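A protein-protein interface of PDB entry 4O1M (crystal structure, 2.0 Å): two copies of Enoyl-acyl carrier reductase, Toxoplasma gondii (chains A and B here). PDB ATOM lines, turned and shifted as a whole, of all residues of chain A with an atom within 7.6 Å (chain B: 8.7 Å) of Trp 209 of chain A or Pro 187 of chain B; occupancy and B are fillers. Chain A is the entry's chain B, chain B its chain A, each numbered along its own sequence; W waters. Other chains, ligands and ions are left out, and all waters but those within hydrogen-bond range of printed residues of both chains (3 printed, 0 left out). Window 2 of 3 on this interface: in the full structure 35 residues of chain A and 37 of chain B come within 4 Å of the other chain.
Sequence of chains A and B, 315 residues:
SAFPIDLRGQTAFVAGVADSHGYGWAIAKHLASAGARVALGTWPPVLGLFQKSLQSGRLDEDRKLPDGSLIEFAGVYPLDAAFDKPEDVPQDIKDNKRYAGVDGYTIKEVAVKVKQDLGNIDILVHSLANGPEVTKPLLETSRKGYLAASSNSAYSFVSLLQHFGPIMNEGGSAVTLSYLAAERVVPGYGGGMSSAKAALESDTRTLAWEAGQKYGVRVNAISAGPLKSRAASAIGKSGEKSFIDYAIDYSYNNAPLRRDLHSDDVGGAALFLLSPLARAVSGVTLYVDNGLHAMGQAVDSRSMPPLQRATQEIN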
ATOM      1  N   ASP A 203     -16.599  24.094  19.076  1.00  0.00           N
ATOM      2  CA  ASP A 203     -16.124  25.130  19.991  1.00  0.00           C
ATOM      3  C   ASP A 203     -16.141  26.529  19.368  1.00  0.00           C
ATOM      4  O   ASP A 203     -16.415  27.490  20.047  1.00  0.00           O
ATOM      5  CB  ASP A 203     -14.720  24.795  20.504  1.00  0.00           C
ATOM      6  CG  ASP A 203     -14.710  23.540  21.393  1.00  0.00           C
ATOM      7  OD1 ASP A 203     -15.826  23.053  21.752  1.00  0.00           O
ATOM      8  OD2 ASP A 203     -13.598  23.001  21.695  1.00  0.00           O
ATOM      9  N   THR A 204     -15.870  26.616  18.068  1.00  0.00           N
ATOM     10  CA  THR A 204     -15.988  27.867  17.339  1.00  0.00           C
ATOM     11  C   THR A 204     -17.422  28.434  17.515  1.00  0.00           C
ATOM     12  O   THR A 204     -17.598  29.620  17.761  1.00  0.00           O
ATOM     13  CB  THR A 204     -15.644  27.617  15.831  1.00  0.00           C
ATOM     14  OG1 THR A 204     -14.282  27.218  15.763  1.00  0.00           O
ATOM     15  CG2 THR A 204     -15.852  28.856  14.976  1.00  0.00           C
ATOM     16  N   ARG A 205     -18.434  27.578  17.371  1.00  0.00           N
ATOM     17  CA  ARG A 205     -19.842  27.981  17.564  1.00  0.00           C
ATOM     18  C   ARG A 205     -20.129  28.327  19.007  1.00  0.00           C
ATOM     19  O   ARG A 205     -20.713  29.377  19.279  1.00  0.00           O
ATOM     20  CB  ARG A 205     -20.816  26.856  17.113  1.00  0.00           C
ATOM     21  CG  ARG A 205     -20.752  26.632  15.605  1.00  0.00           C
ATOM     22  CD  ARG A 205     -21.721  25.552  15.117  1.00  0.00           C
ATOM     23  NE  ARG A 205     -21.377  24.170  15.529  1.00  0.00           N
ATOM     24  CZ  ARG A 205     -20.597  23.357  14.823  1.00  0.00           C
ATOM     25  NH1 ARG A 205     -20.027  23.790  13.698  1.00  0.00           N
ATOM     26  NH2 ARG A 205     -20.376  22.113  15.227  1.00  0.00           N
ATOM     27  N   THR A 206     -19.717  27.463  19.930  1.00  0.00           N
ATOM     28  CA  THR A 206     -19.980  27.743  21.357  1.00  0.00           C
ATOM     29  C   THR A 206     -19.269  29.028  21.833  1.00  0.00           C
ATOM     30  O   THR A 206     -19.847  29.830  22.561  1.00  0.00           O
ATOM     31  CB  THR A 206     -19.503  26.585  22.231  1.00  0.00           C
ATOM     32  OG1 THR A 206     -20.079  25.359  21.748  1.00  0.00           O
ATOM     33  CG2 THR A 206     -19.895  26.839  23.689  1.00  0.00           C
ATOM     34  N   LEU A 207     -18.006  29.211  21.430  1.00  0.00           N
ATOM     35  CA  LEU A 207     -17.259  30.436  21.787  1.00  0.00           C
ATOM     36  C   LEU A 207     -17.818  31.663  21.056  1.00  0.00           C
ATOM     37  O   LEU A 207     -17.776  32.802  21.590  1.00  0.00           O
ATOM     38  CB  LEU A 207     -15.774  30.275  21.435  1.00  0.00           C
ATOM     39  CG  LEU A 207     -15.050  29.190  22.236  1.00  0.00           C
ATOM     40  CD1 LEU A 207     -13.705  28.912  21.565  1.00  0.00           C
ATOM     41  CD2 LEU A 207     -14.808  29.624  23.671  1.00  0.00           C
ATOM     42  N   ALA A 208     -18.366  31.458  19.853  1.00  0.00           N
ATOM     43  CA  ALA A 208     -19.036  32.612  19.154  1.00  0.00           C
ATOM     44  C   ALA A 208     -20.174  33.132  20.033  1.00  0.00           C
ATOM     45  O   ALA A 208     -20.320  34.338  20.214  1.00  0.00           O
ATOM     46  CB  ALA A 208     -19.567  32.220  17.789  1.00  0.00           C
ATOM     47  N   TRP A 209     -20.951  32.213  20.597  1.00  0.00           N
ATOM     48  CA  TRP A 209     -22.016  32.592  21.560  1.00  0.00           C
ATOM     49  C   TRP A 209     -21.384  33.230  22.819  1.00  0.00           C
ATOM     50  O   TRP A 209     -21.729  34.342  23.181  1.00  0.00           O
ATOM     51  CB  TRP A 209     -22.911  31.372  21.909  1.00  0.00           C
ATOM     52  CG  TRP A 209     -23.750  31.619  23.164  1.00  0.00           C
ATOM     53  CD1 TRP A 209     -23.589  31.038  24.392  1.00  0.00           C
ATOM     54  CD2 TRP A 209     -24.825  32.575  23.302  1.00  0.00           C
ATOM     55  NE1 TRP A 209     -24.515  31.573  25.301  1.00  0.00           N
ATOM     56  CE2 TRP A 209     -25.275  32.518  24.653  1.00  0.00           C
ATOM     57  CE3 TRP A 209     -25.449  33.475  22.412  1.00  0.00           C
ATOM     58  CZ2 TRP A 209     -26.318  33.319  25.133  1.00  0.00           C
ATOM     59  CZ3 TRP A 209     -26.490  34.286  22.891  1.00  0.00           C
ATOM     60  CH2 TRP A 209     -26.920  34.192  24.246  1.00  0.00           C
ATOM     61  N   GLU A 210     -20.463  32.525  23.474  1.00  0.00           N
ATOM     62  CA  GLU A 210     -19.956  32.972  24.795  1.00  0.00           C
ATOM     63  C   GLU A 210     -19.150  34.234  24.735  1.00  0.00           C
ATOM     64  O   GLU A 210     -19.379  35.151  25.522  1.00  0.00           O
ATOM     65  CB  GLU A 210     -19.137  31.863  25.473  1.00  0.00           C
ATOM     66  CG  GLU A 210     -20.004  30.668  25.842  1.00  0.00           C
ATOM     67  CD  GLU A 210     -19.285  29.687  26.754  1.00  0.00           C
ATOM     68  OE1 GLU A 210     -18.290  30.109  27.391  1.00  0.00           O
ATOM     69  OE2 GLU A 210     -19.720  28.497  26.844  1.00  0.00           O
ATOM     70  N   ALA A 211     -18.222  34.292  23.780  1.00  0.00           N
ATOM     71  CA  ALA A 211     -17.390  35.475  23.536  1.00  0.00           C
ATOM     72  C   ALA A 211     -18.127  36.603  22.810  1.00  0.00           C
ATOM     73  O   ALA A 211     -17.851  37.784  23.048  1.00  0.00           O
ATOM     74  CB  ALA A 211     -16.123  35.084  22.754  1.00  0.00           C
ATOM     75  N   GLY A 212     -19.106  36.272  21.990  1.00  0.00           N
ATOM     76  CA  GLY A 212     -19.975  37.310  21.439  1.00  0.00           C
ATOM     77  C   GLY A 212     -20.757  38.048  22.525  1.00  0.00           C
ATOM     78  O   GLY A 212     -20.858  39.285  22.518  1.00  0.00           O
ATOM     79  N   GLN A 213     -21.294  37.309  23.481  1.00  0.00           N
ATOM     80  CA  GLN A 213     -22.089  37.932  24.569  1.00  0.00           C
ATOM     81  C   GLN A 213     -21.213  38.645  25.602  1.00  0.00           C
ATOM     82  O   GLN A 213     -21.515  39.763  26.033  1.00  0.00           O
ATOM     83  CB  GLN A 213     -22.943  36.850  25.252  1.00  0.00           C
ATOM     84  CG  GLN A 213     -24.078  36.307  24.326  1.00  0.00           C
ATOM     85  CD  GLN A 213     -25.194  37.338  24.179  1.00  0.00           C
ATOM     86  OE1 GLN A 213     -25.844  37.666  25.142  1.00  0.00           O
ATOM     87  NE2 GLN A 213     -25.376  37.877  22.976  1.00  0.00           N
ATOM     88  N   LYS A 214     -20.119  38.005  25.999  1.00  0.00           N
ATOM     89  CA  LYS A 214     -19.286  38.567  27.038  1.00  0.00           C
ATOM     90  C   LYS A 214     -18.378  39.718  26.574  1.00  0.00           C
ATOM     91  O   LYS A 214     -18.178  40.717  27.308  1.00  0.00           O
ATOM     92  CB  LYS A 214     -18.458  37.449  27.664  1.00  0.00           C
ATOM     93  CG  LYS A 214     -17.690  37.870  28.917  1.00  0.00           C
ATOM     94  CD  LYS A 214     -17.112  36.648  29.606  1.00  0.00           C
ATOM     95  CE  LYS A 214     -16.606  37.000  30.999  1.00  0.00           C
ATOM     96  NZ  LYS A 214     -15.981  35.795  31.608  1.00  0.00           N
ATOM     97  N   TYR A 215     -17.792  39.572  25.382  1.00  0.00           N
ATOM     98  CA  TYR A 215     -16.754  40.522  24.915  1.00  0.00           C
ATOM     99  C   TYR A 215     -17.129  41.285  23.652  1.00  0.00           C
ATOM    100  O   TYR A 215     -16.444  42.229  23.263  1.00  0.00           O
ATOM    101  CB  TYR A 215     -15.446  39.782  24.660  1.00  0.00           C
ATOM    102  CG  TYR A 215     -14.882  39.080  25.882  1.00  0.00           C
ATOM    103  CD1 TYR A 215     -14.671  39.788  27.080  1.00  0.00           C
ATOM    104  CD2 TYR A 215     -14.577  37.713  25.854  1.00  0.00           C
ATOM    105  CE1 TYR A 215     -14.155  39.158  28.209  1.00  0.00           C
ATOM    106  CE2 TYR A 215     -14.038  37.073  26.984  1.00  0.00           C
ATOM    107  CZ  TYR A 215     -13.828  37.806  28.139  1.00  0.00           C
ATOM    108  OH  TYR A 215     -13.327  37.223  29.249  1.00  0.00           O
ATOM    109  N   GLY A 216     -18.201  40.865  22.987  1.00  0.00           N
ATOM    110  CA  GLY A 216     -18.556  41.470  21.701  1.00  0.00           C
ATOM    111  C   GLY A 216     -17.556  41.044  20.627  1.00  0.00           C
ATOM    112  O   GLY A 216     -17.326  41.776  19.668  1.00  0.00           O
ATOM    113  N   VAL A 217     -16.974  39.858  20.801  1.00  0.00           N
ATOM    114  CA  VAL A 217     -15.945  39.328  19.911  1.00  0.00           C
ATOM    115  C   VAL A 217     -16.540  38.246  19.000  1.00  0.00           C
ATOM    116  O   VAL A 217     -17.318  37.420  19.450  1.00  0.00           O
ATOM    117  CB  VAL A 217     -14.744  38.814  20.774  1.00  0.00           C
ATOM    118  CG1 VAL A 217     -13.815  37.842  20.013  1.00  0.00           C
ATOM    119  CG2 VAL A 217     -13.915  40.017  21.263  1.00  0.00           C
ATOM    120  N   VAL A 219     -16.118  34.971  16.425  1.00  0.00           N
ATOM    121  CA  VAL A 219     -15.259  33.775  16.451  1.00  0.00           C
ATOM    122  C   VAL A 219     -15.689  32.903  15.261  1.00  0.00           C
ATOM    123  O   VAL A 219     -16.830  32.490  15.166  1.00  0.00           O
ATOM    124  CB  VAL A 219     -15.467  32.955  17.755  1.00  0.00           C
ATOM    125  CG1 VAL A 219     -14.546  31.745  17.742  1.00  0.00           C
ATOM    126  CG2 VAL A 219     -15.211  33.819  18.964  1.00  0.00           C
ATOM    127  N   SER A 282     -20.247  35.487  12.492  1.00  0.00           N
ATOM    128  CA  SER A 282     -19.705  34.805  13.661  1.00  0.00           C
ATOM    129  C   SER A 282     -20.242  33.392  13.716  1.00  0.00           C
ATOM    130  O   SER A 282     -21.401  33.133  13.318  1.00  0.00           O
ATOM    131  CB  SER A 282     -20.064  35.532  14.978  1.00  0.00           C
ATOM    132  OG  SER A 282     -19.172  35.070  15.999  1.00  0.00           O
ATOM    133  N   GLY A 283     -19.396  32.516  14.261  1.00  0.00           N
ATOM    134  CA  GLY A 283     -19.689  31.089  14.345  1.00  0.00           C
ATOM    135  C   GLY A 283     -19.672  30.300  13.029  1.00  0.00           C
ATOM    136  O   GLY A 283     -20.154  29.156  12.992  1.00  0.00           O
ATOM    137  N   VAL B 134     -19.403  19.974  33.451  1.00  0.00           N
ATOM    138  CA  VAL B 134     -20.591  20.234  32.600  1.00  0.00           C
ATOM    139  C   VAL B 134     -21.381  21.511  32.957  1.00  0.00           C
ATOM    140  O   VAL B 134     -21.951  22.162  32.087  1.00  0.00           O
ATOM    141  CB  VAL B 134     -21.551  18.982  32.548  1.00  0.00           C
ATOM    142  CG1 VAL B 134     -22.237  18.743  33.945  1.00  0.00           C
ATOM    143  CG2 VAL B 134     -22.553  19.109  31.375  1.00  0.00           C
ATOM    144  N   THR B 135     -21.386  21.920  34.215  1.00  0.00           N
ATOM    145  CA  THR B 135     -22.103  23.149  34.572  1.00  0.00           C
ATOM    146  C   THR B 135     -21.285  24.406  34.262  1.00  0.00           C
ATOM    147  O   THR B 135     -21.782  25.513  34.461  1.00  0.00           O
ATOM    148  CB  THR B 135     -22.461  23.186  36.092  1.00  0.00           C
ATOM    149  OG1 THR B 135     -21.254  23.193  36.870  1.00  0.00           O
ATOM    150  CG2 THR B 135     -23.288  21.949  36.487  1.00  0.00           C
ATOM    151  N   LYS B 136     -20.035  24.253  33.799  1.00  0.00           N
ATOM    152  CA  LYS B 136     -19.221  25.443  33.526  1.00  0.00           C
ATOM    153  C   LYS B 136     -19.335  25.846  32.053  1.00  0.00           C
ATOM    154  O   LYS B 136     -19.188  25.003  31.176  1.00  0.00           O
ATOM    155  CB  LYS B 136     -17.753  25.192  33.910  1.00  0.00           C
ATOM    156  CG  LYS B 136     -17.556  24.763  35.345  1.00  0.00           C
ATOM    157  CD  LYS B 136     -17.345  25.955  36.214  1.00  0.00           C
ATOM    158  CE  LYS B 136     -17.874  25.690  37.574  1.00  0.00           C
ATOM    159  NZ  LYS B 136     -18.227  26.976  38.171  1.00  0.00           N
ATOM    160  N   PRO B 137     -19.581  27.142  31.772  1.00  0.00           N
ATOM    161  CA  PRO B 137     -19.392  27.580  30.376  1.00  0.00           C
ATOM    162  C   PRO B 137     -18.002  27.198  29.807  1.00  0.00           C
ATOM    163  O   PRO B 137     -17.016  26.989  30.559  1.00  0.00           O
ATOM    164  CB  PRO B 137     -19.479  29.115  30.462  1.00  0.00           C
ATOM    165  CG  PRO B 137     -20.020  29.449  31.838  1.00  0.00           C
ATOM    166  CD  PRO B 137     -19.732  28.276  32.725  1.00  0.00           C
ATOM    167  N   LEU B 138     -17.889  27.159  28.489  1.00  0.00           N
ATOM    168  CA  LEU B 138     -16.602  26.815  27.875  1.00  0.00           C
ATOM    169  C   LEU B 138     -15.473  27.808  28.231  1.00  0.00           C
ATOM    170  O   LEU B 138     -14.322  27.396  28.464  1.00  0.00           O
ATOM    171  CB  LEU B 138     -16.777  26.681  26.369  1.00  0.00           C
ATOM    172  CG  LEU B 138     -15.813  25.816  25.569  1.00  0.00           C
ATOM    173  CD1 LEU B 138     -15.593  24.408  26.190  1.00  0.00           C
ATOM    174  CD2 LEU B 138     -16.337  25.710  24.144  1.00  0.00           C
ATOM    175  N   LEU B 139     -15.800  29.108  28.335  1.00  0.00           N
ATOM    176  CA  LEU B 139     -14.839  30.097  28.817  1.00  0.00           C
ATOM    177  C   LEU B 139     -14.372  29.876  30.271  1.00  0.00           C
ATOM    178  O   LEU B 139     -13.438  30.513  30.687  1.00  0.00           O
ATOM    179  CB  LEU B 139     -15.392  31.527  28.672  1.00  0.00           C
ATOM    180  CG  LEU B 139     -15.493  31.994  27.204  1.00  0.00           C
ATOM    181  CD1 LEU B 139     -16.127  33.373  27.140  1.00  0.00           C
ATOM    182  CD2 LEU B 139     -14.082  32.014  26.569  1.00  0.00           C
ATOM    183  N   TYR B 179     -26.147  14.589  21.297  1.00  0.00           N
ATOM    184  CA  TYR B 179     -27.089  15.640  21.602  1.00  0.00           C
ATOM    185  C   TYR B 179     -26.803  16.800  20.656  1.00  0.00           C
ATOM    186  O   TYR B 179     -25.645  16.980  20.229  1.00  0.00           O
ATOM    187  CB  TYR B 179     -26.967  16.041  23.084  1.00  0.00           C
ATOM    188  CG  TYR B 179     -27.910  17.163  23.506  1.00  0.00           C
ATOM    189  CD1 TYR B 179     -29.284  17.049  23.308  1.00  0.00           C
ATOM    190  CD2 TYR B 179     -27.417  18.303  24.104  1.00  0.00           C
ATOM    191  CE1 TYR B 179     -30.168  18.071  23.664  1.00  0.00           C
ATOM    192  CE2 TYR B 179     -28.268  19.347  24.505  1.00  0.00           C
ATOM    193  CZ  TYR B 179     -29.633  19.237  24.257  1.00  0.00           C
ATOM    194  OH  TYR B 179     -30.445  20.248  24.669  1.00  0.00           O
ATOM    195  N   ALA B 181     -26.358  19.884  20.993  1.00  0.00           N
ATOM    196  CA  ALA B 181     -25.218  20.732  21.374  1.00  0.00           C
ATOM    197  C   ALA B 181     -23.914  20.492  20.568  1.00  0.00           C
ATOM    198  O   ALA B 181     -23.085  21.411  20.446  1.00  0.00           O
ATOM    199  CB  ALA B 181     -24.953  20.627  22.876  1.00  0.00           C
ATOM    200  N   ARG B 184     -25.059  22.731  17.343  1.00  0.00           N
ATOM    201  CA  ARG B 184     -25.579  24.077  17.575  1.00  0.00           C
ATOM    202  C   ARG B 184     -25.536  24.356  19.036  1.00  0.00           C
ATOM    203  O   ARG B 184     -25.514  23.406  19.838  1.00  0.00           O
ATOM    204  CB  ARG B 184     -26.998  24.253  17.053  1.00  0.00           C
ATOM    205  CG  ARG B 184     -27.021  24.081  15.571  1.00  0.00           C
ATOM    206  CD  ARG B 184     -28.152  24.788  14.890  1.00  0.00           C
ATOM    207  NE  ARG B 184     -29.466  24.220  15.146  1.00  0.00           N
ATOM    208  CZ  ARG B 184     -29.945  23.113  14.597  1.00  0.00           C
ATOM    209  NH1 ARG B 184     -29.188  22.405  13.805  1.00  0.00           N
ATOM    210  NH2 ARG B 184     -31.200  22.714  14.849  1.00  0.00           N
ATOM    211  N   VAL B 185     -25.439  25.636  19.384  1.00  0.00           N
ATOM    212  CA  VAL B 185     -25.094  26.028  20.743  1.00  0.00           C
ATOM    213  C   VAL B 185     -26.301  25.854  21.657  1.00  0.00           C
ATOM    214  O   VAL B 185     -27.364  26.436  21.413  1.00  0.00           O
ATOM    215  CB  VAL B 185     -24.603  27.500  20.822  1.00  0.00           C
ATOM    216  CG1 VAL B 185     -24.290  27.892  22.252  1.00  0.00           C
ATOM    217  CG2 VAL B 185     -23.351  27.739  19.916  1.00  0.00           C
ATOM    218  N   VAL B 186     -26.140  25.037  22.698  1.00  0.00           N
ATOM    219  CA  VAL B 186     -27.154  24.918  23.731  1.00  0.00           C
ATOM    220  C   VAL B 186     -26.562  25.452  25.045  1.00  0.00           C
ATOM    221  O   VAL B 186     -25.752  24.757  25.662  1.00  0.00           O
ATOM    222  CB  VAL B 186     -27.633  23.457  23.870  1.00  0.00           C
ATOM    223  CG1 VAL B 186     -28.706  23.332  25.008  1.00  0.00           C
ATOM    224  CG2 VAL B 186     -28.215  22.932  22.527  1.00  0.00           C
ATOM    225  N   PRO B 187     -26.933  26.692  25.467  1.00  0.00           N
ATOM    226  CA  PRO B 187     -26.390  27.217  26.750  1.00  0.00           C
ATOM    227  C   PRO B 187     -26.642  26.226  27.934  1.00  0.00           C
ATOM    228  O   PRO B 187     -27.711  25.594  28.010  1.00  0.00           O
ATOM    229  CB  PRO B 187     -27.147  28.556  26.952  1.00  0.00           C
ATOM    230  CG  PRO B 187     -27.520  28.982  25.506  1.00  0.00           C
ATOM    231  CD  PRO B 187     -27.836  27.664  24.804  1.00  0.00           C
ATOM    232  N   GLY B 188     -25.652  26.056  28.804  1.00  0.00           N
ATOM    233  CA  GLY B 188     -25.805  25.147  29.938  1.00  0.00           C
ATOM    234  C   GLY B 188     -25.240  23.753  29.724  1.00  0.00           C
ATOM    235  O   GLY B 188     -25.002  23.054  30.695  1.00  0.00           O
ATOM    236  N   TYR B 189     -25.027  23.318  28.472  1.00  0.00           N
ATOM    237  CA  TYR B 189     -24.364  22.027  28.233  1.00  0.00           C
ATOM    238  C   TYR B 189     -22.837  22.299  28.095  1.00  0.00           C
ATOM    239  O   TYR B 189     -22.301  22.430  26.996  1.00  0.00           O
ATOM    240  CB  TYR B 189     -24.940  21.354  26.982  1.00  0.00           C
ATOM    241  CG  TYR B 189     -24.614  19.896  26.886  1.00  0.00           C
ATOM    242  CD1 TYR B 189     -25.050  18.996  27.862  1.00  0.00           C
ATOM    243  CD2 TYR B 189     -23.839  19.409  25.834  1.00  0.00           C
ATOM    244  CE1 TYR B 189     -24.738  17.617  27.750  1.00  0.00           C
ATOM    245  CE2 TYR B 189     -23.546  18.054  25.698  1.00  0.00           C
ATOM    246  CZ  TYR B 189     -23.976  17.173  26.663  1.00  0.00           C
ATOM    247  OH  TYR B 189     -23.691  15.841  26.514  1.00  0.00           O
ATOM    248  N   GLY B 190     -22.169  22.460  29.231  1.00  0.00           N
ATOM    249  CA  GLY B 190     -20.827  23.028  29.251  1.00  0.00           C
ATOM    250  C   GLY B 190     -19.746  21.997  29.479  1.00  0.00           C
ATOM    251  O   GLY B 190     -19.928  20.809  29.189  1.00  0.00           O
ATOM    252  N   SER B 194     -20.196  19.616  24.857  1.00  0.00           N
ATOM    253  CA  SER B 194     -20.657  19.855  23.498  1.00  0.00           C
ATOM    254  C   SER B 194     -19.546  19.418  22.528  1.00  0.00           C
ATOM    255  O   SER B 194     -19.809  18.762  21.501  1.00  0.00           O
ATOM    256  CB  SER B 194     -21.035  21.348  23.291  1.00  0.00           C
ATOM    257  OG  SER B 194     -19.920  22.166  23.635  1.00  0.00           O
ATOM    258  N   PHE B 243     -32.604  22.502  36.131  1.00  0.00           N
ATOM    259  CA  PHE B 243     -32.212  22.728  34.742  1.00  0.00           C
ATOM    260  C   PHE B 243     -32.747  21.735  33.695  1.00  0.00           C
ATOM    261  O   PHE B 243     -33.146  22.139  32.589  1.00  0.00           O
ATOM    262  CB  PHE B 243     -30.702  22.753  34.639  1.00  0.00           C
ATOM    263  CG  PHE B 243     -30.210  23.163  33.290  1.00  0.00           C
ATOM    264  CD1 PHE B 243     -30.304  24.498  32.877  1.00  0.00           C
ATOM    265  CD2 PHE B 243     -29.653  22.227  32.428  1.00  0.00           C
ATOM    266  CE1 PHE B 243     -29.846  24.891  31.612  1.00  0.00           C
ATOM    267  CE2 PHE B 243     -29.194  22.600  31.162  1.00  0.00           C
ATOM    268  CZ  PHE B 243     -29.289  23.939  30.754  1.00  0.00           C
ATOM    269  N   ALA B 247     -35.146  22.363  30.182  1.00  0.00           N
ATOM    270  CA  ALA B 247     -34.772  21.883  28.850  1.00  0.00           C
ATOM    271  C   ALA B 247     -35.915  21.053  28.289  1.00  0.00           C
ATOM    272  O   ALA B 247     -36.246  21.178  27.111  1.00  0.00           O
ATOM    273  CB  ALA B 247     -33.456  21.082  28.862  1.00  0.00           C
ATOM    274  N   TYR B 250     -38.802  23.429  27.304  1.00  0.00           N
ATOM    275  CA  TYR B 250     -38.447  24.126  26.070  1.00  0.00           C
ATOM    276  C   TYR B 250     -38.783  23.232  24.865  1.00  0.00           C
ATOM    277  O   TYR B 250     -39.427  23.678  23.893  1.00  0.00           O
ATOM    278  CB  TYR B 250     -36.961  24.504  26.056  1.00  0.00           C
ATOM    279  CG  TYR B 250     -36.546  25.225  24.791  1.00  0.00           C
ATOM    280  CD1 TYR B 250     -36.228  24.514  23.637  1.00  0.00           C
ATOM    281  CD2 TYR B 250     -36.501  26.644  24.751  1.00  0.00           C
ATOM    282  CE1 TYR B 250     -35.883  25.172  22.440  1.00  0.00           C
ATOM    283  CE2 TYR B 250     -36.147  27.322  23.566  1.00  0.00           C
ATOM    284  CZ  TYR B 250     -35.861  26.578  22.412  1.00  0.00           C
ATOM    285  OH  TYR B 250     -35.486  27.249  21.266  1.00  0.00           O
HETATM  286  O   HOH W   1     -21.693  23.295  18.402  1.00  0.00           O
HETATM  287  O   HOH W   2     -18.594  23.051  21.548  1.00  0.00           O
HETATM  288  O   HOH W   3     -23.135  23.972  22.351  1.00  0.00           O
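The backbone NH (N) of Leu 139 of chain B is in hydrogen-bond range of the side-chain carboxylate (OE1) of Glu 210 of chain A (2.8 Å).
N of Leu 138 of chain B lies within hydrogen-bond range of OE2 of Glu 210 of chain A (2.8 Å).
Asp 203 of chain A touches Leu 138 of chain B.
Val 185 of chain B touches Arg 205 of chain A (CG2 to O, 3.2 Å).
CG2 of Thr 206 of chain A touches CD2 of Leu 138 of chain B (3.8 Å).
Val 185 of chain B touches Thr 206 of chain A (CG2 to N, 3.6 Å).
Thr 206 of chain A touches Ser 194 of chain B (OG1 to OG, 3.7 Å).
Leu 207 of chain A touches Leu 139 of chain B.
CB of Trp 209 of chain A touches CG1 of Val 185 of chain B (3.8 Å).
Trp 209 of chain A touches Pro 187 of chain B (NE1 to CG, 3.97 Å).
CB of Pro 137 of chain B touches OE1 of Glu 210 of chain A, at 3.4 Å.
Of the printed residues of chain B, Asp 203 of chain A touches Leu 138 (3.6 Å).
No residue of chain B comes within 4 Å of Ala 208 of chain A.
Trp 209 of chain A touches just these residues of chain B: Val 185 (3.8 Å) and Pro 187 (3.97 Å).
Printed residues of chain B within 4 Å of Glu 210 of chain A: Pro 137, Leu 138 and Leu 139.
Of the printed residues of chain A, Leu 139 of chain B touches Leu 207 and Glu 210.
Pro 187 of chain B touches one residue of chain A.
Printed residues of chain A within 4 Å of Ser 194 of chain B: Thr 206.
The nearest residue of chain A that does not touch Pro 187 of chain B is Glu 210 of chain A (6.8 Å).
The nearest printed residue of chain B that does not touch Asp 203 of chain A is Ser 194 of chain B (4.6 Å).
Hydrophobic or aromatic side chains of chain B that line the printed part of chain A: Pro 137, Leu 138, Leu 139, Val 185 and Pro 187.
Printed residues of chain A that touch a printed residue of chain B: Asp 203, Arg 205, Thr 206, Leu 207, Trp 209 and Glu 210.
Hydrophobic or aromatic side chains of chain A within 4 Å of the printed part of chain B: Leu 207 and Trp 209.
Along chain A the printed residues that touch a printed residue of chain B span positions 203 to 210.
Among the printed residues, no Asp or Glu carboxylate lies within 4 Å of a Lys or Arg side-chain nitrogen of the other chain.
No position is printed for both chains.
Of the 11 pairs that touch across the chains among the printed residues, none has its exchanged pair printed and touching as well.
Water W2 lies within hydrogen-bond range of the side-chain hydroxyl of Ser 194 of chain B (2.6 Å), the side-chain hydroxyl of Thr 206 of chain A (2.8 Å) and the side-chain carboxylate of Asp 203 of chain A (2.8 Å).
Water W1 bridges the guanidinium group (NE) of Arg 205 of chain A (3.0 Å) and the backbone carbonyl oxygen (O) of Ala 181 of chain B (3.1 Å).
Water W3 lies within hydrogen-bond range of O of Ala 181 of chain B (3.2 Å), N of Val 186 of chain B (3.2 Å) and OG1 of Thr 206 of chain A (3.4 Å).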
